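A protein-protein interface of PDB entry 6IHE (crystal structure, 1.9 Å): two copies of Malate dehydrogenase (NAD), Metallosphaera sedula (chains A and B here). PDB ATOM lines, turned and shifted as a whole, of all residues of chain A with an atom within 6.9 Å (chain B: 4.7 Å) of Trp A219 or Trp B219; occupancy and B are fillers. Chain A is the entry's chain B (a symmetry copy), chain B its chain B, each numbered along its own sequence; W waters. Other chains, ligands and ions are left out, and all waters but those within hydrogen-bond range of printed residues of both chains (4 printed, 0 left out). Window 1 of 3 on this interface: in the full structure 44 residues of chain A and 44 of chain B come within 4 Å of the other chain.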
ATOM      1  N   GLY A   9       3.475   6.093 -17.516  1.00  0.00           N
ATOM      2  CA  GLY A   9       2.689   6.874 -16.579  1.00  0.00           C
ATOM      3  C   GLY A   9       1.213   6.937 -17.028  1.00  0.00           C
ATOM      4  O   GLY A   9       0.723   6.074 -17.803  1.00  0.00           O
ATOM      5  N   LYS A  10       0.544   8.004 -16.628  1.00  0.00           N
ATOM      6  CA  LYS A  10      -0.904   8.155 -16.847  1.00  0.00           C
ATOM      7  C   LYS A  10      -1.234   8.107 -18.310  1.00  0.00           C
ATOM      8  O   LYS A  10      -2.003   7.280 -18.738  1.00  0.00           O
ATOM      9  CB  LYS A  10      -1.412   9.478 -16.231  1.00  0.00           C
ATOM     10  CG  LYS A  10      -1.489   9.437 -14.687  1.00  0.00           C
ATOM     11  CD  LYS A  10      -2.283  10.584 -14.034  1.00  0.00           C
ATOM     12  CE  LYS A  10      -1.913  11.990 -14.499  1.00  0.00           C
ATOM     13  NZ  LYS A  10      -0.478  12.296 -14.233  1.00  0.00           N
ATOM     14  N   ILE A  11      -0.607   8.991 -19.091  1.00  0.00           N
ATOM     15  CA  ILE A  11      -0.861   9.010 -20.486  1.00  0.00           C
ATOM     16  C   ILE A  11      -0.276   7.833 -21.233  1.00  0.00           C
ATOM     17  O   ILE A  11      -0.850   7.364 -22.239  1.00  0.00           O
ATOM     18  CB  ILE A  11      -0.403  10.337 -21.140  1.00  0.00           C
ATOM     19  CG1 ILE A  11      -0.951  10.442 -22.539  1.00  0.00           C
ATOM     20  CG2 ILE A  11       1.119  10.447 -21.228  1.00  0.00           C
ATOM     21  CD1 ILE A  11      -2.449  10.485 -22.551  1.00  0.00           C
ATOM     22  N   GLY A  12       0.875   7.335 -20.807  1.00  0.00           N
ATOM     23  CA  GLY A  12       1.442   6.196 -21.504  1.00  0.00           C
ATOM     24  C   GLY A  12       0.553   4.971 -21.354  1.00  0.00           C
ATOM     25  O   GLY A  12       0.308   4.226 -22.327  1.00  0.00           O
ATOM     26  N   GLN A  13       0.125   4.717 -20.136  1.00  0.00           N
ATOM     27  CA  GLN A  13      -0.798   3.593 -19.899  1.00  0.00           C
ATOM     28  C   GLN A  13      -2.093   3.769 -20.703  1.00  0.00           C
ATOM     29  O   GLN A  13      -2.544   2.826 -21.305  1.00  0.00           O
ATOM     30  CB  GLN A  13      -1.165   3.475 -18.437  1.00  0.00           C
ATOM     31  CG  GLN A  13      -0.053   2.874 -17.605  1.00  0.00           C
ATOM     32  CD  GLN A  13      -0.416   2.793 -16.153  1.00  0.00           C
ATOM     33  OE1 GLN A  13      -1.566   2.486 -15.784  1.00  0.00           O
ATOM     34  NE2 GLN A  13       0.557   3.084 -15.302  1.00  0.00           N
ATOM     35  N   THR A  14      -2.604   5.005 -20.797  1.00  0.00           N
ATOM     36  CA  THR A  14      -3.879   5.196 -21.490  1.00  0.00           C
ATOM     37  C   THR A  14      -3.735   4.945 -22.974  1.00  0.00           C
ATOM     38  O   THR A  14      -4.547   4.251 -23.568  1.00  0.00           O
ATOM     39  CB  THR A  14      -4.498   6.574 -21.246  1.00  0.00           C
ATOM     40  OG1 THR A  14      -4.594   6.806 -19.865  1.00  0.00           O
ATOM     41  CG2 THR A  14      -5.898   6.681 -21.839  1.00  0.00           C
ATOM     42  N   ILE A  15      -2.683   5.484 -23.584  1.00  0.00           N
ATOM     43  CA  ILE A  15      -2.429   5.252 -24.988  1.00  0.00           C
ATOM     44  C   ILE A  15      -2.274   3.775 -25.272  1.00  0.00           C
ATOM     45  O   ILE A  15      -2.864   3.285 -26.225  1.00  0.00           O
ATOM     46  CB  ILE A  15      -1.175   5.951 -25.502  1.00  0.00           C
ATOM     47  CG1 ILE A  15      -1.375   7.484 -25.447  1.00  0.00           C
ATOM     48  CG2 ILE A  15      -0.868   5.496 -26.910  1.00  0.00           C
ATOM     49  CD1 ILE A  15      -0.097   8.289 -25.502  1.00  0.00           C
ATOM     50  N   TYR A  17      -3.244   1.100 -23.513  1.00  0.00           N
ATOM     51  CA  TYR A  17      -4.498   0.375 -23.295  1.00  0.00           C
ATOM     52  C   TYR A  17      -5.409   0.575 -24.468  1.00  0.00           C
ATOM     53  O   TYR A  17      -5.973  -0.351 -25.004  1.00  0.00           O
ATOM     54  CB  TYR A  17      -5.209   0.898 -22.013  1.00  0.00           C
ATOM     55  CG  TYR A  17      -6.583   0.290 -21.829  1.00  0.00           C
ATOM     56  CD1 TYR A  17      -6.718  -0.971 -21.297  1.00  0.00           C
ATOM     57  CD2 TYR A  17      -7.733   0.944 -22.260  1.00  0.00           C
ATOM     58  CE1 TYR A  17      -7.949  -1.525 -21.137  1.00  0.00           C
ATOM     59  CE2 TYR A  17      -8.997   0.396 -22.114  1.00  0.00           C
ATOM     60  CZ  TYR A  17      -9.120  -0.841 -21.552  1.00  0.00           C
ATOM     61  OH  TYR A  17     -10.381  -1.395 -21.376  1.00  0.00           O
ATOM     62  N   SER A  18      -5.566   1.821 -24.891  1.00  0.00           N
ATOM     63  CA  SER A  18      -6.505   2.118 -25.925  1.00  0.00           C
ATOM     64  C   SER A  18      -6.079   1.578 -27.280  1.00  0.00           C
ATOM     65  O   SER A  18      -6.923   1.153 -28.065  1.00  0.00           O
ATOM     66  CB  SER A  18      -6.747   3.676 -25.934  1.00  0.00           C
ATOM     67  OG  SER A  18      -7.462   4.116 -27.069  1.00  0.00           O
ATOM     68  N   PHE A  41       1.565  -3.155 -14.743  1.00  0.00           N
ATOM     69  CA  PHE A  41       0.736  -2.765 -15.852  1.00  0.00           C
ATOM     70  C   PHE A  41       0.515  -3.893 -16.827  1.00  0.00           C
ATOM     71  O   PHE A  41      -0.592  -4.097 -17.323  1.00  0.00           O
ATOM     72  CB  PHE A  41       1.348  -1.542 -16.535  1.00  0.00           C
ATOM     73  CG  PHE A  41       0.580  -1.053 -17.714  1.00  0.00           C
ATOM     74  CD1 PHE A  41      -0.822  -0.889 -17.652  1.00  0.00           C
ATOM     75  CD2 PHE A  41       1.247  -0.666 -18.881  1.00  0.00           C
ATOM     76  CE1 PHE A  41      -1.510  -0.383 -18.744  1.00  0.00           C
ATOM     77  CE2 PHE A  41       0.557  -0.174 -19.978  1.00  0.00           C
ATOM     78  CZ  PHE A  41      -0.818  -0.012 -19.908  1.00  0.00           C
ATOM     79  N   GLU A  44      -2.103  -6.097 -15.366  1.00  0.00           N
ATOM     80  CA  GLU A  44      -3.366  -5.419 -15.633  1.00  0.00           C
ATOM     81  C   GLU A  44      -3.890  -5.639 -17.026  1.00  0.00           C
ATOM     82  O   GLU A  44      -5.065  -5.923 -17.200  1.00  0.00           O
ATOM     83  CB  GLU A  44      -3.204  -3.904 -15.429  1.00  0.00           C
ATOM     84  CG  GLU A  44      -3.161  -3.482 -13.975  1.00  0.00           C
ATOM     85  CD  GLU A  44      -4.555  -3.173 -13.401  1.00  0.00           C
ATOM     86  OE1 GLU A  44      -5.546  -3.944 -13.656  1.00  0.00           O
ATOM     87  OE2 GLU A  44      -4.588  -2.193 -12.642  1.00  0.00           O
ATOM     88  N   LEU A  45      -3.019  -5.457 -18.038  1.00  0.00           N
ATOM     89  CA  LEU A  45      -3.375  -5.697 -19.418  1.00  0.00           C
ATOM     90  C   LEU A  45      -3.751  -7.135 -19.666  1.00  0.00           C
ATOM     91  O   LEU A  45      -4.711  -7.412 -20.325  1.00  0.00           O
ATOM     92  CB  LEU A  45      -2.229  -5.299 -20.342  1.00  0.00           C
ATOM     93  CG  LEU A  45      -2.058  -3.794 -20.424  1.00  0.00           C
ATOM     94  CD1 LEU A  45      -0.761  -3.462 -21.188  1.00  0.00           C
ATOM     95  CD2 LEU A  45      -3.279  -3.223 -21.136  1.00  0.00           C
ATOM     96  N   HIS A  47      -5.104  -9.195 -17.635  1.00  0.00           N
ATOM     97  CA  HIS A  47      -6.407  -9.465 -17.012  1.00  0.00           C
ATOM     98  C   HIS A  47      -7.512  -8.928 -17.913  1.00  0.00           C
ATOM     99  O   HIS A  47      -8.438  -9.602 -18.203  1.00  0.00           O
ATOM    100  CB  HIS A  47      -6.467  -8.812 -15.676  1.00  0.00           C
ATOM    101  CG  HIS A  47      -5.445  -9.288 -14.726  1.00  0.00           C
ATOM    102  ND1 HIS A  47      -5.024  -8.520 -13.666  1.00  0.00           N
ATOM    103  CD2 HIS A  47      -4.655 -10.387 -14.741  1.00  0.00           C
ATOM    104  CE1 HIS A  47      -4.085  -9.166 -13.010  1.00  0.00           C
ATOM    105  NE2 HIS A  47      -3.816 -10.283 -13.663  1.00  0.00           N
ATOM    106  N   ALA A  48      -7.333  -7.722 -18.416  1.00  0.00           N
ATOM    107  CA  ALA A  48      -8.249  -7.153 -19.354  1.00  0.00           C
ATOM    108  C   ALA A  48      -8.383  -7.960 -20.609  1.00  0.00           C
ATOM    109  O   ALA A  48      -9.505  -8.136 -21.144  1.00  0.00           O
ATOM    110  CB  ALA A  48      -7.819  -5.723 -19.683  1.00  0.00           C
ATOM    111  N   PHE A  49      -7.249  -8.415 -21.165  1.00  0.00           N
ATOM    112  CA  PHE A  49      -7.279  -9.219 -22.377  1.00  0.00           C
ATOM    113  C   PHE A  49      -8.089 -10.494 -22.232  1.00  0.00           C
ATOM    114  O   PHE A  49      -8.714 -10.927 -23.199  1.00  0.00           O
ATOM    115  CB  PHE A  49      -5.879  -9.617 -22.839  1.00  0.00           C
ATOM    116  CG  PHE A  49      -4.972  -8.463 -23.282  1.00  0.00           C
ATOM    117  CD1 PHE A  49      -5.434  -7.172 -23.423  1.00  0.00           C
ATOM    118  CD2 PHE A  49      -3.618  -8.728 -23.603  1.00  0.00           C
ATOM    119  CE1 PHE A  49      -4.590  -6.160 -23.835  1.00  0.00           C
ATOM    120  CE2 PHE A  49      -2.778  -7.711 -24.062  1.00  0.00           C
ATOM    121  CZ  PHE A  49      -3.272  -6.445 -24.146  1.00  0.00           C
ATOM    122  N   ILE A 214      -8.457  17.378 -12.294  1.00  0.00           N
ATOM    123  CA  ILE A 214      -8.238  15.908 -12.230  1.00  0.00           C
ATOM    124  C   ILE A 214      -6.797  15.616 -11.947  1.00  0.00           C
ATOM    125  O   ILE A 214      -6.475  14.613 -11.301  1.00  0.00           O
ATOM    126  CB  ILE A 214      -8.715  15.200 -13.537  1.00  0.00           C
ATOM    127  CG1 ILE A 214     -10.178  15.557 -13.790  1.00  0.00           C
ATOM    128  CG2 ILE A 214      -8.564  13.680 -13.433  1.00  0.00           C
ATOM    129  CD1 ILE A 214     -10.728  15.076 -15.118  1.00  0.00           C
ATOM    130  N   GLY A 216      -4.325  15.728 -14.551  1.00  0.00           N
ATOM    131  CA  GLY A 216      -3.623  15.518 -15.818  1.00  0.00           C
ATOM    132  C   GLY A 216      -4.628  15.044 -16.829  1.00  0.00           C
ATOM    133  O   GLY A 216      -5.667  14.518 -16.439  1.00  0.00           O
ATOM    134  N   THR A 217      -4.337  15.265 -18.105  1.00  0.00           N
ATOM    135  CA  THR A 217      -5.215  14.806 -19.176  1.00  0.00           C
ATOM    136  C   THR A 217      -4.910  13.362 -19.490  1.00  0.00           C
ATOM    137  O   THR A 217      -3.749  12.931 -19.424  1.00  0.00           O
ATOM    138  CB  THR A 217      -5.118  15.672 -20.416  1.00  0.00           C
ATOM    139  OG1 THR A 217      -3.733  15.778 -20.807  1.00  0.00           O
ATOM    140  CG2 THR A 217      -5.767  17.063 -20.142  1.00  0.00           C
ATOM    141  N   THR A 218      -5.956  12.575 -19.760  1.00  0.00           N
ATOM    142  CA  THR A 218      -5.787  11.121 -20.013  1.00  0.00           C
ATOM    143  C   THR A 218      -6.590  10.526 -21.142  1.00  0.00           C
ATOM    144  O   THR A 218      -6.041  10.254 -22.212  1.00  0.00           O
ATOM    145  CB  THR A 218      -6.039  10.319 -18.745  1.00  0.00           C
ATOM    146  OG1 THR A 218      -7.327  10.633 -18.193  1.00  0.00           O
ATOM    147  CG2 THR A 218      -4.963  10.614 -17.753  1.00  0.00           C
ATOM    148  N   TRP A 219      -7.905  10.366 -20.931  1.00  0.00           N
ATOM    149  CA  TRP A 219      -8.785   9.645 -21.851  1.00  0.00           C
ATOM    150  C   TRP A 219      -8.846  10.301 -23.211  1.00  0.00           C
ATOM    151  O   TRP A 219      -8.831   9.631 -24.272  1.00  0.00           O
ATOM    152  CB  TRP A 219     -10.215   9.490 -21.295  1.00  0.00           C
ATOM    153  CG  TRP A 219     -10.232   8.972 -19.949  1.00  0.00           C
ATOM    154  CD1 TRP A 219     -10.444   9.689 -18.838  1.00  0.00           C
ATOM    155  CD2 TRP A 219      -9.950   7.633 -19.520  1.00  0.00           C
ATOM    156  NE1 TRP A 219     -10.339   8.898 -17.732  1.00  0.00           N
ATOM    157  CE2 TRP A 219     -10.042   7.619 -18.129  1.00  0.00           C
ATOM    158  CE3 TRP A 219      -9.592   6.456 -20.175  1.00  0.00           C
ATOM    159  CZ2 TRP A 219      -9.815   6.482 -17.373  1.00  0.00           C
ATOM    160  CZ3 TRP A 219      -9.386   5.295 -19.392  1.00  0.00           C
ATOM    161  CH2 TRP A 219      -9.512   5.329 -18.034  1.00  0.00           C
ATOM    162  N   GLY A 220      -8.908  11.602 -23.222  1.00  0.00           N
ATOM    163  CA  GLY A 220      -9.018  12.286 -24.539  1.00  0.00           C
ATOM    164  C   GLY A 220      -7.744  12.117 -25.421  1.00  0.00           C
ATOM    165  O   GLY A 220      -7.767  11.496 -26.499  1.00  0.00           O
ATOM    166  N   PRO A 221      -6.605  12.648 -24.955  1.00  0.00           N
ATOM    167  CA  PRO A 221      -5.376  12.505 -25.778  1.00  0.00           C
ATOM    168  C   PRO A 221      -4.961  11.075 -25.894  1.00  0.00           C
ATOM    169  O   PRO A 221      -4.444  10.667 -26.893  1.00  0.00           O
ATOM    170  CB  PRO A 221      -4.320  13.344 -25.025  1.00  0.00           C
ATOM    171  CG  PRO A 221      -4.907  13.591 -23.685  1.00  0.00           C
ATOM    172  CD  PRO A 221      -6.403  13.560 -23.823  1.00  0.00           C
ATOM    173  N   GLY A 222      -5.235  10.276 -24.889  1.00  0.00           N
ATOM    174  CA  GLY A 222      -4.908   8.892 -24.993  1.00  0.00           C
ATOM    175  C   GLY A 222      -5.582   8.191 -26.152  1.00  0.00           C
ATOM    176  O   GLY A 222      -4.937   7.395 -26.880  1.00  0.00           O
ATOM    177  N   THR A 223      -6.915   8.422 -26.302  1.00  0.00           N
ATOM    178  CA  THR A 223      -7.704   7.839 -27.380  1.00  0.00           C
ATOM    179  C   THR A 223      -7.289   8.444 -28.709  1.00  0.00           C
ATOM    180  O   THR A 223      -7.190   7.727 -29.754  1.00  0.00           O
ATOM    181  CB  THR A 223      -9.226   8.029 -27.127  1.00  0.00           C
ATOM    182  OG1 THR A 223      -9.574   7.500 -25.807  1.00  0.00           O
ATOM    183  CG2 THR A 223     -10.025   7.329 -28.190  1.00  0.00           C
ATOM    184  N   ILE A 224      -7.127   9.771 -28.714  1.00  0.00           N
ATOM    185  CA  ILE A 224      -6.770  10.435 -29.938  1.00  0.00           C
ATOM    186  C   ILE A 224      -5.368   9.963 -30.496  1.00  0.00           C
ATOM    187  O   ILE A 224      -5.234   9.684 -31.702  1.00  0.00           O
ATOM    188  CB  ILE A 224      -6.805  11.954 -29.688  1.00  0.00           C
ATOM    189  CG1 ILE A 224      -8.262  12.410 -29.503  1.00  0.00           C
ATOM    190  CG2 ILE A 224      -6.133  12.680 -30.834  1.00  0.00           C
ATOM    191  CD1 ILE A 224      -8.410  13.731 -28.788  1.00  0.00           C
ATOM    192  N   GLN B  13     -13.996   6.001 -13.655  1.00  0.00           N
ATOM    193  CA  GLN B  13     -13.625   6.531 -14.980  1.00  0.00           C
ATOM    194  C   GLN B  13     -13.224   5.397 -15.931  1.00  0.00           C
ATOM    195  O   GLN B  13     -13.653   5.396 -17.060  1.00  0.00           O
ATOM    196  CB  GLN B  13     -12.467   7.498 -14.885  1.00  0.00           C
ATOM    197  CG  GLN B  13     -12.880   8.849 -14.343  1.00  0.00           C
ATOM    198  CD  GLN B  13     -11.718   9.789 -14.222  1.00  0.00           C
ATOM    199  OE1 GLN B  13     -10.818   9.827 -15.084  1.00  0.00           O
ATOM    200  NE2 GLN B  13     -11.708  10.552 -13.140  1.00  0.00           N
ATOM    201  N   THR B  14     -12.503   4.385 -15.426  1.00  0.00           N
ATOM    202  CA  THR B  14     -12.037   3.328 -16.322  1.00  0.00           C
ATOM    203  C   THR B  14     -13.192   2.494 -16.828  1.00  0.00           C
ATOM    204  O   THR B  14     -13.285   2.216 -18.013  1.00  0.00           O
ATOM    205  CB  THR B  14     -10.973   2.428 -15.691  1.00  0.00           C
ATOM    206  OG1 THR B  14      -9.923   3.219 -15.198  1.00  0.00           O
ATOM    207  CG2 THR B  14     -10.388   1.446 -16.700  1.00  0.00           C
ATOM    208  N   TYR B  17     -15.243   4.665 -19.356  1.00  0.00           N
ATOM    209  CA  TYR B  17     -14.522   4.818 -20.622  1.00  0.00           C
ATOM    210  C   TYR B  17     -14.608   3.547 -21.411  1.00  0.00           C
ATOM    211  O   TYR B  17     -14.913   3.542 -22.583  1.00  0.00           O
ATOM    212  CB  TYR B  17     -13.023   5.140 -20.354  1.00  0.00           C
ATOM    213  CG  TYR B  17     -12.202   5.155 -21.626  1.00  0.00           C
ATOM    214  CD1 TYR B  17     -12.214   6.258 -22.447  1.00  0.00           C
ATOM    215  CD2 TYR B  17     -11.483   4.039 -22.042  1.00  0.00           C
ATOM    216  CE1 TYR B  17     -11.484   6.274 -23.594  1.00  0.00           C
ATOM    217  CE2 TYR B  17     -10.738   4.029 -23.211  1.00  0.00           C
ATOM    218  CZ  TYR B  17     -10.730   5.143 -23.998  1.00  0.00           C
ATOM    219  OH  TYR B  17      -9.970   5.159 -25.160  1.00  0.00           O
ATOM    220  N   PHE B  41     -14.240  15.156 -16.696  1.00  0.00           N
ATOM    221  CA  PHE B  41     -14.272  13.842 -17.281  1.00  0.00           C
ATOM    222  C   PHE B  41     -15.163  13.776 -18.495  1.00  0.00           C
ATOM    223  O   PHE B  41     -14.822  13.160 -19.503  1.00  0.00           O
ATOM    224  CB  PHE B  41     -14.692  12.825 -16.218  1.00  0.00           C
ATOM    225  CG  PHE B  41     -14.774  11.423 -16.714  1.00  0.00           C
ATOM    226  CD1 PHE B  41     -13.740  10.866 -17.497  1.00  0.00           C
ATOM    227  CD2 PHE B  41     -15.844  10.603 -16.339  1.00  0.00           C
ATOM    228  CE1 PHE B  41     -13.814   9.542 -17.903  1.00  0.00           C
ATOM    229  CE2 PHE B  41     -15.925   9.285 -16.758  1.00  0.00           C
ATOM    230  CZ  PHE B  41     -14.904   8.744 -17.522  1.00  0.00           C
ATOM    231  N   GLU B  44     -13.247  15.228 -21.334  1.00  0.00           N
ATOM    232  CA  GLU B  44     -12.336  14.172 -21.760  1.00  0.00           C
ATOM    233  C   GLU B  44     -12.975  13.144 -22.654  1.00  0.00           C
ATOM    234  O   GLU B  44     -12.405  12.778 -23.671  1.00  0.00           O
ATOM    235  CB  GLU B  44     -11.770  13.437 -20.534  1.00  0.00           C
ATOM    236  CG  GLU B  44     -10.699  14.212 -19.795  1.00  0.00           C
ATOM    237  CD  GLU B  44      -9.284  13.926 -20.326  1.00  0.00           C
ATOM    238  OE1 GLU B  44      -9.063  13.870 -21.587  1.00  0.00           O
ATOM    239  OE2 GLU B  44      -8.415  13.841 -19.444  1.00  0.00           O
ATOM    240  N   ALA B  48     -12.328  12.228 -26.761  1.00  0.00           N
ATOM    241  CA  ALA B  48     -12.126  10.892 -27.228  1.00  0.00           C
ATOM    242  C   ALA B  48     -13.145  10.462 -28.239  1.00  0.00           C
ATOM    243  O   ALA B  48     -12.808   9.796 -29.248  1.00  0.00           O
ATOM    244  CB  ALA B  48     -12.118   9.932 -26.037  1.00  0.00           C
ATOM    245  N   THR B 217      -5.929  -0.679  -8.597  1.00  0.00           N
ATOM    246  CA  THR B 217      -6.206  -1.460  -9.798  1.00  0.00           C
ATOM    247  C   THR B 217      -7.130  -0.679 -10.700  1.00  0.00           C
ATOM    248  O   THR B 217      -8.016   0.047 -10.224  1.00  0.00           O
ATOM    249  CB  THR B 217      -6.772  -2.829  -9.479  1.00  0.00           C
ATOM    250  OG1 THR B 217      -7.915  -2.676  -8.612  1.00  0.00           O
ATOM    251  CG2 THR B 217      -5.665  -3.727  -8.851  1.00  0.00           C
ATOM    252  N   THR B 218      -6.889  -0.756 -12.012  1.00  0.00           N
ATOM    253  CA  THR B 218      -7.685   0.025 -12.993  1.00  0.00           C
ATOM    254  C   THR B 218      -8.098  -0.686 -14.258  1.00  0.00           C
ATOM    255  O   THR B 218      -9.262  -1.072 -14.395  1.00  0.00           O
ATOM    256  CB  THR B 218      -6.975   1.320 -13.359  1.00  0.00           C
ATOM    257  OG1 THR B 218      -5.641   1.053 -13.823  1.00  0.00           O
ATOM    258  CG2 THR B 218      -6.939   2.216 -12.167  1.00  0.00           C
ATOM    259  N   TRP B 219      -7.140  -0.908 -15.168  1.00  0.00           N
ATOM    260  CA  TRP B 219      -7.411  -1.422 -16.513  1.00  0.00           C
ATOM    261  C   TRP B 219      -8.025  -2.802 -16.479  1.00  0.00           C
ATOM    262  O   TRP B 219      -8.967  -3.127 -17.242  1.00  0.00           O
ATOM    263  CB  TRP B 219      -6.148  -1.446 -17.397  1.00  0.00           C
ATOM    264  CG  TRP B 219      -5.442  -0.188 -17.387  1.00  0.00           C
ATOM    265  CD1 TRP B 219      -4.319   0.072 -16.706  1.00  0.00           C
ATOM    266  CD2 TRP B 219      -5.827   1.040 -18.019  1.00  0.00           C
ATOM    267  NE1 TRP B 219      -3.948   1.373 -16.877  1.00  0.00           N
ATOM    268  CE2 TRP B 219      -4.862   1.990 -17.693  1.00  0.00           C
ATOM    269  CE3 TRP B 219      -6.913   1.435 -18.797  1.00  0.00           C
ATOM    270  CZ2 TRP B 219      -4.924   3.304 -18.125  1.00  0.00           C
ATOM    271  CZ3 TRP B 219      -6.954   2.775 -19.254  1.00  0.00           C
ATOM    272  CH2 TRP B 219      -5.970   3.660 -18.925  1.00  0.00           C
ATOM    273  N   GLY B 220      -7.526  -3.635 -15.611  1.00  0.00           N
ATOM    274  CA  GLY B 220      -8.070  -5.020 -15.579  1.00  0.00           C
ATOM    275  C   GLY B 220      -9.558  -5.081 -15.117  1.00  0.00           C
ATOM    276  O   GLY B 220     -10.468  -5.460 -15.875  1.00  0.00           O
ATOM    277  N   PRO B 221      -9.824  -4.675 -13.867  1.00  0.00           N
ATOM    278  CA  PRO B 221     -11.234  -4.726 -13.398  1.00  0.00           C
ATOM    279  C   PRO B 221     -12.096  -3.776 -14.163  1.00  0.00           C
ATOM    280  O   PRO B 221     -13.239  -4.040 -14.396  1.00  0.00           O
ATOM    281  CB  PRO B 221     -11.147  -4.339 -11.906  1.00  0.00           C
ATOM    282  CG  PRO B 221      -9.791  -3.761 -11.734  1.00  0.00           C
ATOM    283  CD  PRO B 221      -8.894  -4.372 -12.772  1.00  0.00           C
ATOM    284  N   GLY B 222     -11.541  -2.675 -14.616  1.00  0.00           N
ATOM    285  CA  GLY B 222     -12.321  -1.777 -15.402  1.00  0.00           C
ATOM    286  C   GLY B 222     -12.878  -2.397 -16.665  1.00  0.00           C
ATOM    287  O   GLY B 222     -14.069  -2.187 -17.009  1.00  0.00           O
ATOM    288  N   THR B 223     -12.004  -3.120 -17.417  1.00  0.00           N
ATOM    289  CA  THR B 223     -12.389  -3.798 -18.648  1.00  0.00           C
ATOM    290  C   THR B 223     -13.319  -4.955 -18.332  1.00  0.00           C
ATOM    291  O   THR B 223     -14.324  -5.210 -19.068  1.00  0.00           O
ATOM    292  CB  THR B 223     -11.139  -4.281 -19.438  1.00  0.00           C
ATOM    293  OG1 THR B 223     -10.234  -3.152 -19.660  1.00  0.00           O
ATOM    294  CG2 THR B 223     -11.551  -4.878 -20.754  1.00  0.00           C
HETATM  295  O   HOH W   1      -8.031  13.052 -17.086  1.00  0.00           O
HETATM  296  O   HOH W   2      -3.586   0.085 -12.271  1.00  0.00           O
HETATM  297  O   HOH W   3     -10.662  12.040 -16.570  1.00  0.00           O
HETATM  298  O   HOH W   4      -1.852   0.133 -14.553  1.00  0.00           O
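Water W2 bridges the side-chain carboxylate (OE2) of Glu A44 (2.5 Å) and the side-chain hydroxyl (OG1) of Thr B218 (2.8 Å).
Water W4 bridges the side-chain amide oxygen (OE1) of Gln A13 and the indole nitrogen (NE1) of Trp B219.
O of Trp B219 is in hydrogen-bond range of OG1 of Thr B223, at 2.7 Å.
The side-chain hydroxyl of Thr A14 is in hydrogen-bond range of the backbone carbonyl oxygen of Lys A10, at 2.9 Å.
The side-chain hydroxyl of Thr A223 is in hydrogen-bond range of the backbone carbonyl oxygen of Trp A219, 2.7 Å away.
Among the printed residues, merely in contact across the chains: Trp A219 with Tyr B17 (3.3 Å), Tyr A17 with Trp B219 (3.3 Å), Thr A217 with Glu B44 (3.4 Å), Glu A44 with Thr B217 (3.4 Å), Pro A221 with Glu B44 (3.5 Å), Glu A44 with Pro B221 (3.5 Å), Phe A41 with Trp B219 (3.5 Å), Trp A219 with Phe B41 (3.5 Å), Trp A219 with Trp B219 (3.5 Å), Thr A223 with Ala B48 (3.5 Å), Ala A48 with Thr B223 (3.5 Å), Trp A219 with Thr B14 (3.6 Å), Thr A14 with Trp B219 (3.6 Å), Trp A219 with Ala B48 (3.7 Å), Ala A48 with Trp B219 (3.7 Å), Glu A44 with Trp B219 (3.7 Å), Trp A219 with Glu B44 (3.7 Å), Ile A214 with Phe B41 (3.9 Å), Ala A48 with Gly B220 (3.99 Å) and Gly A220 with Ala B48 (3.99 Å).
Of the printed residues of chain B, Tyr A17 touches Trp B219 (3.3 Å) and Thr B223 (2.5 Å).
Of the printed residues of chain B, Thr A218 touches Glu B44.
Trp A219 touches seven residues of chain B.
Of the printed residues of chain A, Ala B48 touches Trp A219 (3.7 Å), Gly A220 (3.99 Å) and Thr A223 (3.5 Å).
Printed residues of chain A within 4 Å of Thr B217: Glu A44 (3.4 Å).
Trp B219 touches just these residues of chain A: Gln A13, Thr A14, Tyr A17, Phe A41, Glu A44, Ala A48 and Trp A219.
The nearest printed residue of chain B that does not touch Trp A219 is Thr B218 (6.7 Å).
The nearest residue of chain A that does not touch Trp B219 is Lys A10 (5.0 Å).
The nearest printed residue of chain B that does not touch Ser A18 is Trp B219 (5.9 Å).
Hydrophobic or aromatic side chains of chain B that line the printed part of chain A: Tyr B17, Phe B41, Ala B48, Trp B219 and Pro B221.
Along chain B the printed residues that touch a printed residue of chain A span positions 13 to 223.
Printed residues of chain A that touch a printed residue of chain B: Gln A13, Thr A14, Tyr A17, Ser A18, Phe A41, Glu A44, Ala A48, Ile A214, Thr A217, Thr A218, Trp A219, Gly A220, Pro A221 and Thr A223.
Among the printed residues, no Asp or Glu carboxylate lies within 4 Å of a Lys or Arg side-chain nitrogen of the other chain.
The indole nitrogen of Trp A219 is in hydrogen-bond range of the side-chain amide oxygen of Gln B13 (2.8 Å).
The side-chain hydroxyl (OG) of Ser A18 is in hydrogen-bond range of the side-chain hydroxyl (OH) of Tyr B17 (3.3 Å).
OH of Tyr B17 lies within hydrogen-bond range of OG1 of Thr A223, 2.5 Å away.
The side-chain carboxylate of Glu B44 lies within hydrogen-bond range of the backbone NH of Thr A218, at 2.8 Å.
The side-chain carboxylate (OE1) of Glu B44 sits at hydrogen-bond distance from the backbone NH (N) of Gly A220 (2.8 Å).
N of Thr B218 is in hydrogen-bond range of OE2 of Glu A44.
NE1 of Trp B219 sits at hydrogen-bond distance from OE1 of Gln A13 (2.8 Å).
The backbone NH of Gly B220 sits at hydrogen-bond distance from the side-chain carboxylate of Glu A44 (2.8 Å).
The side-chain hydroxyl (OH) of Tyr A17 sits at hydrogen-bond distance from the side-chain hydroxyl (OG1) of Thr B223 (2.5 Å).
Tyr A17 touches Trp B219, and with the chains exchanged Trp A219 touches Tyr B17.
Glu A44 touches Trp B219, and with the chains exchanged Trp A219 touches Glu B44.
Glu A44 touches Gly B220, and with the chains exchanged Gly A220 touches Glu B44.
Trp B219 touches its own counterpart, Trp A219.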
